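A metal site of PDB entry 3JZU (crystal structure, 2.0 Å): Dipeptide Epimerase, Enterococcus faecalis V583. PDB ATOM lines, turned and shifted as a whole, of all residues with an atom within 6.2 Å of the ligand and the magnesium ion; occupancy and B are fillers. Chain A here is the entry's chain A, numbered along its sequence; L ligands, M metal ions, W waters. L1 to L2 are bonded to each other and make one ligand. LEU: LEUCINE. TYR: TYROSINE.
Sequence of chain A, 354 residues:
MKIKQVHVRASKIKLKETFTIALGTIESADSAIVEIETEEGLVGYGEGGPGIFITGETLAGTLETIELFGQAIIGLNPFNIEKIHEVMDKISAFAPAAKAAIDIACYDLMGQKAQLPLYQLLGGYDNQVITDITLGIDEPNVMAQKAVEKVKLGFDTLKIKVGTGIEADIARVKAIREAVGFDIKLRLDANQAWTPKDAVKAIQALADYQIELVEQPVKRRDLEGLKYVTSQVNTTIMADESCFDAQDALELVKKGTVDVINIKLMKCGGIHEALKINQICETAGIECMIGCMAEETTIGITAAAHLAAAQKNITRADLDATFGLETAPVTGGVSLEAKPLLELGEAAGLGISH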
ATOM      1  N   LEU A  15      22.712   9.677  -0.215  1.00  0.00           N
ATOM      2  CA  LEU A  15      22.423   8.936   1.011  1.00  0.00           C
ATOM      3  C   LEU A  15      23.497   7.860   1.124  1.00  0.00           C
ATOM      4  O   LEU A  15      23.989   7.376   0.101  1.00  0.00           O
ATOM      5  CB  LEU A  15      21.036   8.281   0.961  1.00  0.00           C
ATOM      6  CG  LEU A  15      19.829   9.221   0.831  1.00  0.00           C
ATOM      7  CD1 LEU A  15      18.548   8.416   1.026  1.00  0.00           C
ATOM      8  CD2 LEU A  15      19.914  10.323   1.863  1.00  0.00           C
ATOM      9  N   PHE A  19      17.532   3.430  -0.050  1.00  0.00           N
ATOM     10  CA  PHE A  19      16.506   2.973   0.863  1.00  0.00           C
ATOM     11  C   PHE A  19      15.334   2.440   0.064  1.00  0.00           C
ATOM     12  O   PHE A  19      14.798   3.142  -0.791  1.00  0.00           O
ATOM     13  CB  PHE A  19      16.031   4.116   1.757  1.00  0.00           C
ATOM     14  CG  PHE A  19      15.855   3.723   3.186  1.00  0.00           C
ATOM     15  CD1 PHE A  19      16.960   3.588   4.023  1.00  0.00           C
ATOM     16  CD2 PHE A  19      14.591   3.459   3.705  1.00  0.00           C
ATOM     17  CE1 PHE A  19      16.804   3.195   5.352  1.00  0.00           C
ATOM     18  CE2 PHE A  19      14.423   3.062   5.027  1.00  0.00           C
ATOM     19  CZ  PHE A  19      15.534   2.930   5.849  1.00  0.00           C
ATOM     20  N   ILE A  21      11.458   0.974  -0.028  1.00  0.00           N
ATOM     21  CA  ILE A  21      10.172   0.858   0.646  1.00  0.00           C
ATOM     22  C   ILE A  21       9.259   0.251  -0.410  1.00  0.00           C
ATOM     23  O   ILE A  21       9.679   0.060  -1.557  1.00  0.00           O
ATOM     24  CB  ILE A  21       9.611   2.209   1.136  1.00  0.00           C
ATOM     25  CG1 ILE A  21       9.359   3.163  -0.038  1.00  0.00           C
ATOM     26  CG2 ILE A  21      10.595   2.854   2.128  1.00  0.00           C
ATOM     27  CD1 ILE A  21       8.599   4.402   0.365  1.00  0.00           C
ATOM     28  N   LEU A  23       6.943   1.510  -2.110  1.00  0.00           N
ATOM     29  CA  LEU A  23       6.725   2.459  -3.217  1.00  0.00           C
ATOM     30  C   LEU A  23       7.885   2.635  -4.208  1.00  0.00           C
ATOM     31  O   LEU A  23       7.681   3.116  -5.322  1.00  0.00           O
ATOM     32  CB  LEU A  23       6.356   3.814  -2.646  1.00  0.00           C
ATOM     33  CG  LEU A  23       5.144   3.793  -1.701  1.00  0.00           C
ATOM     34  CD1 LEU A  23       4.955   5.157  -1.059  1.00  0.00           C
ATOM     35  CD2 LEU A  23       3.904   3.360  -2.460  1.00  0.00           C
ATOM     36  N   THR A  25      12.501   3.284  -4.471  1.00  0.00           N
ATOM     37  CA  THR A  25      13.767   3.535  -3.788  1.00  0.00           C
ATOM     38  C   THR A  25      14.087   5.007  -3.756  1.00  0.00           C
ATOM     39  O   THR A  25      13.543   5.800  -4.533  1.00  0.00           O
ATOM     40  CB  THR A  25      14.918   2.827  -4.502  1.00  0.00           C
ATOM     41  OG1 THR A  25      15.003   3.319  -5.850  1.00  0.00           O
ATOM     42  CG2 THR A  25      14.701   1.303  -4.517  1.00  0.00           C
ATOM     43  N   ILE A  26      14.979   5.380  -2.839  1.00  0.00           N
ATOM     44  CA  ILE A  26      15.428   6.756  -2.709  1.00  0.00           C
ATOM     45  C   ILE A  26      16.935   6.631  -2.478  1.00  0.00           C
ATOM     46  O   ILE A  26      17.388   5.793  -1.687  1.00  0.00           O
ATOM     47  CB  ILE A  26      14.737   7.454  -1.516  1.00  0.00           C
ATOM     48  CG1 ILE A  26      14.898   8.976  -1.618  1.00  0.00           C
ATOM     49  CG2 ILE A  26      15.288   6.941  -0.205  1.00  0.00           C
ATOM     50  CD1 ILE A  26      16.314   9.473  -1.443  1.00  0.00           C
ATOM     51  N   PRO A  50      10.665  17.323  -1.013  1.00  0.00           N
ATOM     52  CA  PRO A  50       9.609  16.539  -1.640  1.00  0.00           C
ATOM     53  C   PRO A  50       9.883  15.054  -1.906  1.00  0.00           C
ATOM     54  O   PRO A  50      10.966  14.683  -2.354  1.00  0.00           O
ATOM     55  CB  PRO A  50       9.352  17.295  -2.931  1.00  0.00           C
ATOM     56  CG  PRO A  50      10.753  17.646  -3.358  1.00  0.00           C
ATOM     57  CD  PRO A  50      11.429  18.081  -2.032  1.00  0.00           C
ATOM     58  N   GLY A  51       8.871  14.235  -1.650  1.00  0.00           N
ATOM     59  CA  GLY A  51       8.966  12.802  -1.904  1.00  0.00           C
ATOM     60  C   GLY A  51       8.026  12.546  -3.071  1.00  0.00           C
ATOM     61  O   GLY A  51       6.806  12.511  -2.880  1.00  0.00           O
ATOM     62  N   ILE A  52       8.592  12.365  -4.260  1.00  0.00           N
ATOM     63  CA  ILE A  52       7.811  12.159  -5.461  1.00  0.00           C
ATOM     64  C   ILE A  52       6.802  10.997  -5.392  1.00  0.00           C
ATOM     65  O   ILE A  52       5.672  11.156  -5.831  1.00  0.00           O
ATOM     66  CB  ILE A  52       8.733  11.991  -6.710  1.00  0.00           C
ATOM     67  CG1 ILE A  52       7.909  12.081  -7.995  1.00  0.00           C
ATOM     68  CG2 ILE A  52       9.510  10.685  -6.635  1.00  0.00           C
ATOM     69  CD1 ILE A  52       8.739  12.207  -9.268  1.00  0.00           C
ATOM     70  N   PHE A  53       7.192   9.861  -4.823  1.00  0.00           N
ATOM     71  CA  PHE A  53       6.213   8.782  -4.776  1.00  0.00           C
ATOM     72  C   PHE A  53       5.229   8.905  -3.615  1.00  0.00           C
ATOM     73  O   PHE A  53       4.485   7.976  -3.323  1.00  0.00           O
ATOM     74  CB  PHE A  53       6.886   7.394  -4.828  1.00  0.00           C
ATOM     75  CG  PHE A  53       8.008   7.193  -3.847  1.00  0.00           C
ATOM     76  CD1 PHE A  53       9.156   6.497  -4.245  1.00  0.00           C
ATOM     77  CD2 PHE A  53       7.913   7.624  -2.531  1.00  0.00           C
ATOM     78  CE1 PHE A  53      10.177   6.227  -3.330  1.00  0.00           C
ATOM     79  CE2 PHE A  53       8.927   7.368  -1.610  1.00  0.00           C
ATOM     80  CZ  PHE A  53      10.063   6.667  -2.014  1.00  0.00           C
ATOM     81  N   ILE A  54       5.212  10.069  -2.979  1.00  0.00           N
ATOM     82  CA  ILE A  54       4.270  10.314  -1.891  1.00  0.00           C
ATOM     83  C   ILE A  54       3.314  11.444  -2.282  1.00  0.00           C
ATOM     84  O   ILE A  54       2.103  11.279  -2.254  1.00  0.00           O
ATOM     85  CB  ILE A  54       4.991  10.728  -0.587  1.00  0.00           C
ATOM     86  CG1 ILE A  54       5.892   9.583  -0.115  1.00  0.00           C
ATOM     87  CG2 ILE A  54       3.959  11.043   0.492  1.00  0.00           C
ATOM     88  CD1 ILE A  54       5.120   8.309   0.227  1.00  0.00           C
ATOM     89  N   ASP A 132      12.704   6.693  16.467  1.00  0.00           N
ATOM     90  CA  ASP A 132      12.975   5.309  16.117  1.00  0.00           C
ATOM     91  C   ASP A 132      13.929   5.442  14.940  1.00  0.00           C
ATOM     92  O   ASP A 132      14.402   6.550  14.630  1.00  0.00           O
ATOM     93  CB  ASP A 132      11.690   4.591  15.650  1.00  0.00           C
ATOM     94  CG  ASP A 132      11.076   5.214  14.395  1.00  0.00           C
ATOM     95  OD1 ASP A 132      11.814   5.758  13.548  1.00  0.00           O
ATOM     96  OD2 ASP A 132       9.830   5.148  14.240  1.00  0.00           O
ATOM     97  N   THR A 134      14.269   3.643  10.952  1.00  0.00           N
ATOM     98  CA  THR A 134      13.653   2.761   9.965  1.00  0.00           C
ATOM     99  C   THR A 134      14.666   1.841   9.282  1.00  0.00           C
ATOM    100  O   THR A 134      15.778   2.269   8.963  1.00  0.00           O
ATOM    101  CB  THR A 134      12.939   3.576   8.870  1.00  0.00           C
ATOM    102  OG1 THR A 134      11.945   4.426   9.471  1.00  0.00           O
ATOM    103  CG2 THR A 134      12.251   2.644   7.847  1.00  0.00           C
ATOM    104  N   LYS A 159      11.520   0.778  13.164  1.00  0.00           N
ATOM    105  CA  LYS A 159      10.426   0.863  12.198  1.00  0.00           C
ATOM    106  C   LYS A 159      10.798  -0.063  11.054  1.00  0.00           C
ATOM    107  O   LYS A 159      11.797   0.170  10.357  1.00  0.00           O
ATOM    108  CB  LYS A 159      10.243   2.303  11.705  1.00  0.00           C
ATOM    109  CG  LYS A 159       9.139   2.463  10.672  1.00  0.00           C
ATOM    110  CD  LYS A 159       8.809   3.942  10.442  1.00  0.00           C
ATOM    111  CE  LYS A 159       7.800   4.114   9.319  1.00  0.00           C
ATOM    112  NZ  LYS A 159       7.369   5.541   9.110  1.00  0.00           N
ATOM    113  N   LYS A 161      10.141  -1.755   7.450  1.00  0.00           N
ATOM    114  CA  LYS A 161       9.469  -1.576   6.180  1.00  0.00           C
ATOM    115  C   LYS A 161       9.130  -2.956   5.655  1.00  0.00           C
ATOM    116  O   LYS A 161       9.939  -3.881   5.741  1.00  0.00           O
ATOM    117  CB  LYS A 161      10.374  -0.828   5.204  1.00  0.00           C
ATOM    118  CG  LYS A 161      10.544   0.647   5.535  1.00  0.00           C
ATOM    119  CD  LYS A 161       9.244   1.424   5.300  1.00  0.00           C
ATOM    120  CE  LYS A 161       9.390   2.888   5.715  1.00  0.00           C
ATOM    121  NZ  LYS A 161       8.131   3.669   5.479  1.00  0.00           N
ATOM    122  N   ASP A 189       5.613  -0.796   8.736  1.00  0.00           N
ATOM    123  CA  ASP A 189       5.121   0.183   7.774  1.00  0.00           C
ATOM    124  C   ASP A 189       5.049  -0.505   6.416  1.00  0.00           C
ATOM    125  O   ASP A 189       6.086  -0.808   5.831  1.00  0.00           O
ATOM    126  CB  ASP A 189       6.045   1.404   7.678  1.00  0.00           C
ATOM    127  CG  ASP A 189       5.435   2.523   6.851  1.00  0.00           C
ATOM    128  OD1 ASP A 189       4.496   2.239   6.071  1.00  0.00           O
ATOM    129  OD2 ASP A 189       5.883   3.688   6.978  1.00  0.00           O
ATOM    130  N   ASN A 191       3.618   0.806   3.666  1.00  0.00           N
ATOM    131  CA  ASN A 191       3.479   1.776   2.586  1.00  0.00           C
ATOM    132  C   ASN A 191       2.451   1.357   1.528  1.00  0.00           C
ATOM    133  O   ASN A 191       2.777   1.288   0.342  1.00  0.00           O
ATOM    134  CB  ASN A 191       4.844   2.094   1.949  1.00  0.00           C
ATOM    135  CG  ASN A 191       5.692   3.025   2.813  1.00  0.00           C
ATOM    136  OD1 ASN A 191       6.745   2.629   3.332  1.00  0.00           O
ATOM    137  ND2 ASN A 191       5.221   4.254   2.985  1.00  0.00           N
ATOM    138  N   GLU A 215       1.714   0.681  10.152  1.00  0.00           N
ATOM    139  CA  GLU A 215       1.474   1.931   9.441  1.00  0.00           C
ATOM    140  C   GLU A 215       0.979   1.709   8.000  1.00  0.00           C
ATOM    141  O   GLU A 215       1.496   0.857   7.278  1.00  0.00           O
ATOM    142  CB  GLU A 215       2.772   2.736   9.421  1.00  0.00           C
ATOM    143  CG  GLU A 215       2.620   4.178   9.026  1.00  0.00           C
ATOM    144  CD  GLU A 215       3.915   4.953   9.193  1.00  0.00           C
ATOM    145  OE1 GLU A 215       4.808   4.481   9.941  1.00  0.00           O
ATOM    146  OE2 GLU A 215       4.030   6.042   8.600  1.00  0.00           O
ATOM    147  N   GLN A 216      -0.037   2.474   7.607  1.00  0.00           N
ATOM    148  CA  GLN A 216      -0.652   2.435   6.276  1.00  0.00           C
ATOM    149  C   GLN A 216      -0.609   1.081   5.569  1.00  0.00           C
ATOM    150  O   GLN A 216       0.101   0.910   4.577  1.00  0.00           O
ATOM    151  CB  GLN A 216       0.003   3.509   5.391  1.00  0.00           C
ATOM    152  CG  GLN A 216      -0.793   3.921   4.155  1.00  0.00           C
ATOM    153  CD  GLN A 216      -2.134   4.560   4.479  1.00  0.00           C
ATOM    154  OE1 GLN A 216      -2.223   5.514   5.262  1.00  0.00           O
ATOM    155  NE2 GLN A 216      -3.180   4.038   3.882  1.00  0.00           N
ATOM    156  N   ASP A 240      -0.800   7.071   7.217  1.00  0.00           N
ATOM    157  CA  ASP A 240       0.281   7.946   6.791  1.00  0.00           C
ATOM    158  C   ASP A 240      -0.148   8.590   5.490  1.00  0.00           C
ATOM    159  O   ASP A 240      -0.622   9.716   5.485  1.00  0.00           O
ATOM    160  CB  ASP A 240       1.584   7.189   6.606  1.00  0.00           C
ATOM    161  CG  ASP A 240       2.718   8.076   6.135  1.00  0.00           C
ATOM    162  OD1 ASP A 240       2.546   9.325   6.125  1.00  0.00           O
ATOM    163  OD2 ASP A 240       3.791   7.538   5.779  1.00  0.00           O
ATOM    164  N   GLU A 241       0.016   7.877   4.376  1.00  0.00           N
ATOM    165  CA  GLU A 241      -0.372   8.454   3.093  1.00  0.00           C
ATOM    166  C   GLU A 241      -1.857   8.818   3.047  1.00  0.00           C
ATOM    167  O   GLU A 241      -2.243   9.730   2.314  1.00  0.00           O
ATOM    168  CB  GLU A 241      -0.025   7.506   1.934  1.00  0.00           C
ATOM    169  CG  GLU A 241       1.467   7.320   1.727  1.00  0.00           C
ATOM    170  CD  GLU A 241       2.001   6.080   2.419  1.00  0.00           C
ATOM    171  OE1 GLU A 241       1.634   5.844   3.585  1.00  0.00           O
ATOM    172  OE2 GLU A 241       2.780   5.339   1.793  1.00  0.00           O
ATOM    173  N   ASN A 262       0.182   9.705  11.294  1.00  0.00           N
ATOM    174  CA  ASN A 262       1.554  10.131  10.997  1.00  0.00           C
ATOM    175  C   ASN A 262       1.537  11.550  10.427  1.00  0.00           C
ATOM    176  O   ASN A 262       0.928  11.799   9.386  1.00  0.00           O
ATOM    177  CB  ASN A 262       2.183   9.183   9.959  1.00  0.00           C
ATOM    178  CG  ASN A 262       3.632   9.547   9.608  1.00  0.00           C
ATOM    179  OD1 ASN A 262       3.927  10.695   9.269  1.00  0.00           O
ATOM    180  ND2 ASN A 262       4.538   8.565   9.682  1.00  0.00           N
ATOM    181  N   LYS A 264       3.614  14.764   8.814  1.00  0.00           N
ATOM    182  CA  LYS A 264       4.860  15.150   8.129  1.00  0.00           C
ATOM    183  C   LYS A 264       4.698  16.598   7.686  1.00  0.00           C
ATOM    184  O   LYS A 264       3.692  16.949   7.063  1.00  0.00           O
ATOM    185  CB  LYS A 264       5.136  14.276   6.906  1.00  0.00           C
ATOM    186  CG  LYS A 264       5.597  12.861   7.209  1.00  0.00           C
ATOM    187  CD  LYS A 264       5.953  12.120   5.946  1.00  0.00           C
ATOM    188  CE  LYS A 264       6.221  10.651   6.221  1.00  0.00           C
ATOM    189  NZ  LYS A 264       5.034  10.030   6.854  1.00  0.00           N
ATOM    190  N   MET A 289       2.198  10.670  15.447  1.00  0.00           N
ATOM    191  CA  MET A 289       3.621  10.402  15.367  1.00  0.00           C
ATOM    192  C   MET A 289       4.152  11.389  14.351  1.00  0.00           C
ATOM    193  O   MET A 289       3.538  11.597  13.300  1.00  0.00           O
ATOM    194  CB  MET A 289       3.912   8.984  14.877  1.00  0.00           C
ATOM    195  CG  MET A 289       5.413   8.748  14.626  1.00  0.00           C
ATOM    196  SD  MET A 289       5.826   7.030  14.204  1.00  0.00           S
ATOM    197  CE  MET A 289       5.727   7.048  12.449  1.00  0.00           C
ATOM    198  N   GLY A 291       6.687  12.336  11.515  1.00  0.00           N
ATOM    199  CA  GLY A 291       7.501  11.577  10.579  1.00  0.00           C
ATOM    200  C   GLY A 291       8.309  12.457   9.643  1.00  0.00           C
ATOM    201  O   GLY A 291       8.433  13.652   9.879  1.00  0.00           O
ATOM    202  N   CYS A 292       8.851  11.865   8.589  1.00  0.00           N
ATOM    203  CA  CYS A 292       9.662  12.646   7.641  1.00  0.00           C
ATOM    204  C   CYS A 292       9.871  11.945   6.306  1.00  0.00           C
ATOM    205  O   CYS A 292       9.663  10.738   6.157  1.00  0.00           O
ATOM    206  CB  CYS A 292      11.037  12.932   8.252  1.00  0.00           C
ATOM    207  SG  CYS A 292      12.031  11.446   8.527  1.00  0.00           S
ATOM    208  N   MET A 293      10.309  12.741   5.332  1.00  0.00           N
ATOM    209  CA  MET A 293      10.622  12.248   4.001  1.00  0.00           C
ATOM    210  C   MET A 293      12.124  11.960   4.056  1.00  0.00           C
ATOM    211  O   MET A 293      12.835  12.575   4.834  1.00  0.00           O
ATOM    212  CB  MET A 293      10.353  13.333   2.954  1.00  0.00           C
ATOM    213  CG  MET A 293       8.913  13.794   2.910  1.00  0.00           C
ATOM    214  SD  MET A 293       7.800  12.427   2.543  1.00  0.00           S
ATOM    215  CE  MET A 293       6.272  13.328   2.170  1.00  0.00           C
ATOM    216  N   ALA A 294      12.606  11.026   3.237  1.00  0.00           N
ATOM    217  CA  ALA A 294      14.032  10.718   3.228  1.00  0.00           C
ATOM    218  C   ALA A 294      14.812  11.889   2.612  1.00  0.00           C
ATOM    219  O   ALA A 294      15.997  12.071   2.891  1.00  0.00           O
ATOM    220  CB  ALA A 294      14.293   9.438   2.422  1.00  0.00           C
ATOM    221  N   GLU A 295      14.118  12.690   1.807  1.00  0.00           N
ATOM    222  CA  GLU A 295      14.730  13.836   1.129  1.00  0.00           C
ATOM    223  C   GLU A 295      14.982  15.076   2.000  1.00  0.00           C
ATOM    224  O   GLU A 295      15.528  16.074   1.534  1.00  0.00           O
ATOM    225  CB  GLU A 295      13.858  14.239  -0.072  1.00  0.00           C
ATOM    226  CG  GLU A 295      13.773  13.182  -1.167  1.00  0.00           C
ATOM    227  CD  GLU A 295      12.671  12.161  -0.946  1.00  0.00           C
ATOM    228  OE1 GLU A 295      12.182  12.022   0.203  1.00  0.00           O
ATOM    229  OE2 GLU A 295      12.292  11.487  -1.925  1.00  0.00           O
ATOM    230  N   ASP A 318       9.528   9.543  14.278  1.00  0.00           N
ATOM    231  CA  ASP A 318      10.251   8.803  13.246  1.00  0.00           C
ATOM    232  C   ASP A 318      10.956   9.895  12.446  1.00  0.00           C
ATOM    233  O   ASP A 318      10.533  10.258  11.338  1.00  0.00           O
ATOM    234  CB  ASP A 318       9.254   8.029  12.371  1.00  0.00           C
ATOM    235  CG  ASP A 318       9.925   7.332  11.182  1.00  0.00           C
ATOM    236  OD1 ASP A 318      10.958   6.678  11.385  1.00  0.00           O
ATOM    237  OD2 ASP A 318       9.402   7.441  10.050  1.00  0.00           O
ATOM    238  N   LEU A 319      12.022  10.446  13.032  1.00  0.00           N
ATOM    239  CA  LEU A 319      12.817  11.513  12.416  1.00  0.00           C
ATOM    240  C   LEU A 319      14.241  10.992  12.261  1.00  0.00           C
ATOM    241  O   LEU A 319      15.135  11.337  13.051  1.00  0.00           O
ATOM    242  CB  LEU A 319      12.800  12.744  13.323  1.00  0.00           C
ATOM    243  CG  LEU A 319      11.390  13.237  13.646  1.00  0.00           C
ATOM    244  CD1 LEU A 319      11.416  14.400  14.631  1.00  0.00           C
ATOM    245  CD2 LEU A 319      10.711  13.639  12.339  1.00  0.00           C
ATOM    246  N   ASP A 320      14.436  10.185  11.221  1.00  0.00           N
ATOM    247  CA  ASP A 320      15.718   9.552  10.954  1.00  0.00           C
ATOM    248  C   ASP A 320      16.326   9.913   9.594  1.00  0.00           C
ATOM    249  O   ASP A 320      17.260   9.251   9.144  1.00  0.00           O
ATOM    250  CB  ASP A 320      15.541   8.029  11.074  1.00  0.00           C
ATOM    251  CG  ASP A 320      14.413   7.479  10.202  1.00  0.00           C
ATOM    252  OD1 ASP A 320      13.615   8.283   9.672  1.00  0.00           O
ATOM    253  OD2 ASP A 320      14.307   6.238  10.062  1.00  0.00           O
ATOM    254  N   ALA A 321      15.822  10.948   8.947  1.00  0.00           N
ATOM    255  CA  ALA A 321      16.374  11.320   7.653  1.00  0.00           C
ATOM    256  C   ALA A 321      17.849  11.724   7.702  1.00  0.00           C
ATOM    257  O   ALA A 321      18.607  11.408   6.774  1.00  0.00           O
ATOM    258  CB  ALA A 321      15.548  12.430   7.015  1.00  0.00           C
ATOM    259  N   THR A 322      18.276  12.412   8.757  1.00  0.00           N
ATOM    260  CA  THR A 322      19.669  12.853   8.840  1.00  0.00           C
ATOM    261  C   THR A 322      20.661  11.727   9.015  1.00  0.00           C
ATOM    262  O   THR A 322      21.835  11.865   8.630  1.00  0.00           O
ATOM    263  CB  THR A 322      19.920  13.869  10.002  1.00  0.00           C
ATOM    264  OG1 THR A 322      19.685  13.232  11.259  1.00  0.00           O
ATOM    265  CG2 THR A 322      19.031  15.088   9.852  1.00  0.00           C
HETATM  266  N   LEU L   1      11.343   7.234   8.311  1.00  0.00           N
HETATM  267  CA  LEU L   1      11.265   7.667   6.884  1.00  0.00           C
HETATM  268  C   LEU L   1       9.988   7.166   6.212  1.00  0.00           C
HETATM  269  O   LEU L   1       9.591   6.011   6.412  1.00  0.00           O
HETATM  270  CB  LEU L   1      12.471   7.131   6.099  1.00  0.00           C
HETATM  271  CG  LEU L   1      13.888   7.502   6.553  1.00  0.00           C
HETATM  272  CD1 LEU L   1      14.903   6.902   5.604  1.00  0.00           C
HETATM  273  CD2 LEU L   1      14.035   9.016   6.579  1.00  0.00           C
HETATM  274  N   TYR L   2       9.359   8.019   5.407  1.00  0.00           N
HETATM  275  CA  TYR L   2       8.156   7.666   4.662  1.00  0.00           C
HETATM  276  C   TYR L   2       7.132   6.874   5.479  1.00  0.00           C
HETATM  277  O   TYR L   2       6.975   7.172   6.676  1.00  0.00           O
HETATM  278  CB  TYR L   2       8.532   6.854   3.413  1.00  0.00           C
HETATM  279  CG  TYR L   2       9.472   7.571   2.460  1.00  0.00           C
HETATM  280  CD1 TYR L   2      10.538   6.885   1.872  1.00  0.00           C
HETATM  281  CD2 TYR L   2       9.281   8.905   2.103  1.00  0.00           C
HETATM  282  CE1 TYR L   2      11.391   7.519   0.966  1.00  0.00           C
HETATM  283  CE2 TYR L   2      10.124   9.549   1.195  1.00  0.00           C
HETATM  284  CZ  TYR L   2      11.183   8.837   0.624  1.00  0.00           C
HETATM  285  OH  TYR L   2      12.024   9.444  -0.286  1.00  0.00           O
HETATM  286  OXT TYR L   2       6.497   5.957   4.889  1.00  0.00           O
HETATM  287 MG    MG M   1       4.807   5.687   6.676  1.00  0.00          MG
HETATM  288  O   HOH W   1      18.235   7.653   4.865  1.00  0.00           O
HETATM  289  O   HOH W   2       7.736   9.094   8.800  1.00  0.00           O
HETATM  290  O   HOH W   3       3.262   4.667   5.452  1.00  0.00           O
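N of LEU L1 lies within salt-bridge range of OD2 of Asp 318.
The side-chain carboxylate of Glu 295 sits at hydrogen-bond distance from an oxygen (OH) of TYR L2.
The backbone carbonyl oxygen (O) of Cys 292 is in hydrogen-bond range of a nitrogen (N) of TYR L2.
The side-chain carboxylate (OD1) of Asp 320 is in salt-bridge range of a nitrogen (N) of LEU L1, 2.8 Å away.
An oxygen (OXT) of TYR L2 sits close to the side-chain amide nitrogen of Asn 191 (2.9 Å).
O of TYR L2 lies within salt-bridge range of NZ of Lys 161, at 3.9 Å.
O of TYR L2 lies within salt-bridge range of NZ of Lys 159.
OG1 of Thr 134 is in hydrogen-bond range of N of LEU L1.
O of TYR L2 lies within salt-bridge range of NZ of Lys 264, at 3.5 Å.
OD2 of Asp 189 lies close to NZ of Lys 159 (3.2 Å).
OE1 of Gln 216 sits at hydrogen-bond distance from N of Asp 240, 2.9 Å away.
O of Asp 318 sits at hydrogen-bond distance from SG of Cys 292.
The side-chain carboxylate (OD2) of Asp 318 is in salt-bridge range of the side-chain amino group (NZ) of Lys 159 (2.9 Å).
OD1 of Asp 132 sits close to OD1 of Asp 318.
The side-chain carboxylate (OD2) of Asp 320 sits at hydrogen-bond distance from the backbone NH (N) of Thr 134, at 2.7 Å.
The side-chain amide oxygen (OD1) of Asn 191 is in hydrogen-bond range of the side-chain amino group (NZ) of Lys 161 (2.8 Å).
NZ of Lys 264 sits at hydrogen-bond distance from OD1 of Asn 262, 2.7 Å away.
Phe 19 touches the ligand.
CD1 of Ile 21 touches CD1 of TYR L2, 3.5 Å away.
Ile 26 touches the ligand.
CZ of Phe 53 touches CE1 of TYR L2, 3.4 Å away.
SD of Met 293 touches CD2 of TYR L2 (3.8 Å).
Ala 294 touches the ligand.
Ala 321 touches the ligand.
Hydrophobic or aromatic side chains within 4 Å of the ligand: Phe 19, Ile 21, Ile 26, Phe 53, Met 293, Ala 294 and Ala 321.
Of the 34 residues printed, 19 come within 4 Å of the ligand.
Along chain A the residues within 4 Å of the ligand span positions 19 to 321.
The nearest printed residue that does not touch the ligand is Ile 54 (4.1 Å).
Lys 159 touches the magnesium ion.
Asn 191 touches the magnesium ion (ND2 to MG, 3.98 Å).
The nearest printed residue that does not touch the magnesium ion is Lys 161 (4.1 Å).
The magnesium ion is bound by OE2 of Glu 215 (2.1 Å), water W3 (2.2 Å), OD2 of Asp 189 (2.3 Å), OD2 of Asp 240 (2.3 Å) and OXT of TYR L2 (2.5 Å).
The magnesium ion has five donor atoms within binding distance.
Slightly farther from the magnesium ion lies O of TYR L2 (2.6 Å).
Water W3 lies within hydrogen-bond range of the side-chain carboxylate (OE1) of Glu 241 (2.7 Å), the side-chain carboxylate (OD1) of Asp 189 (2.8 Å) and the side-chain amide nitrogen (ND2) of Asn 191 (3.2 Å).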
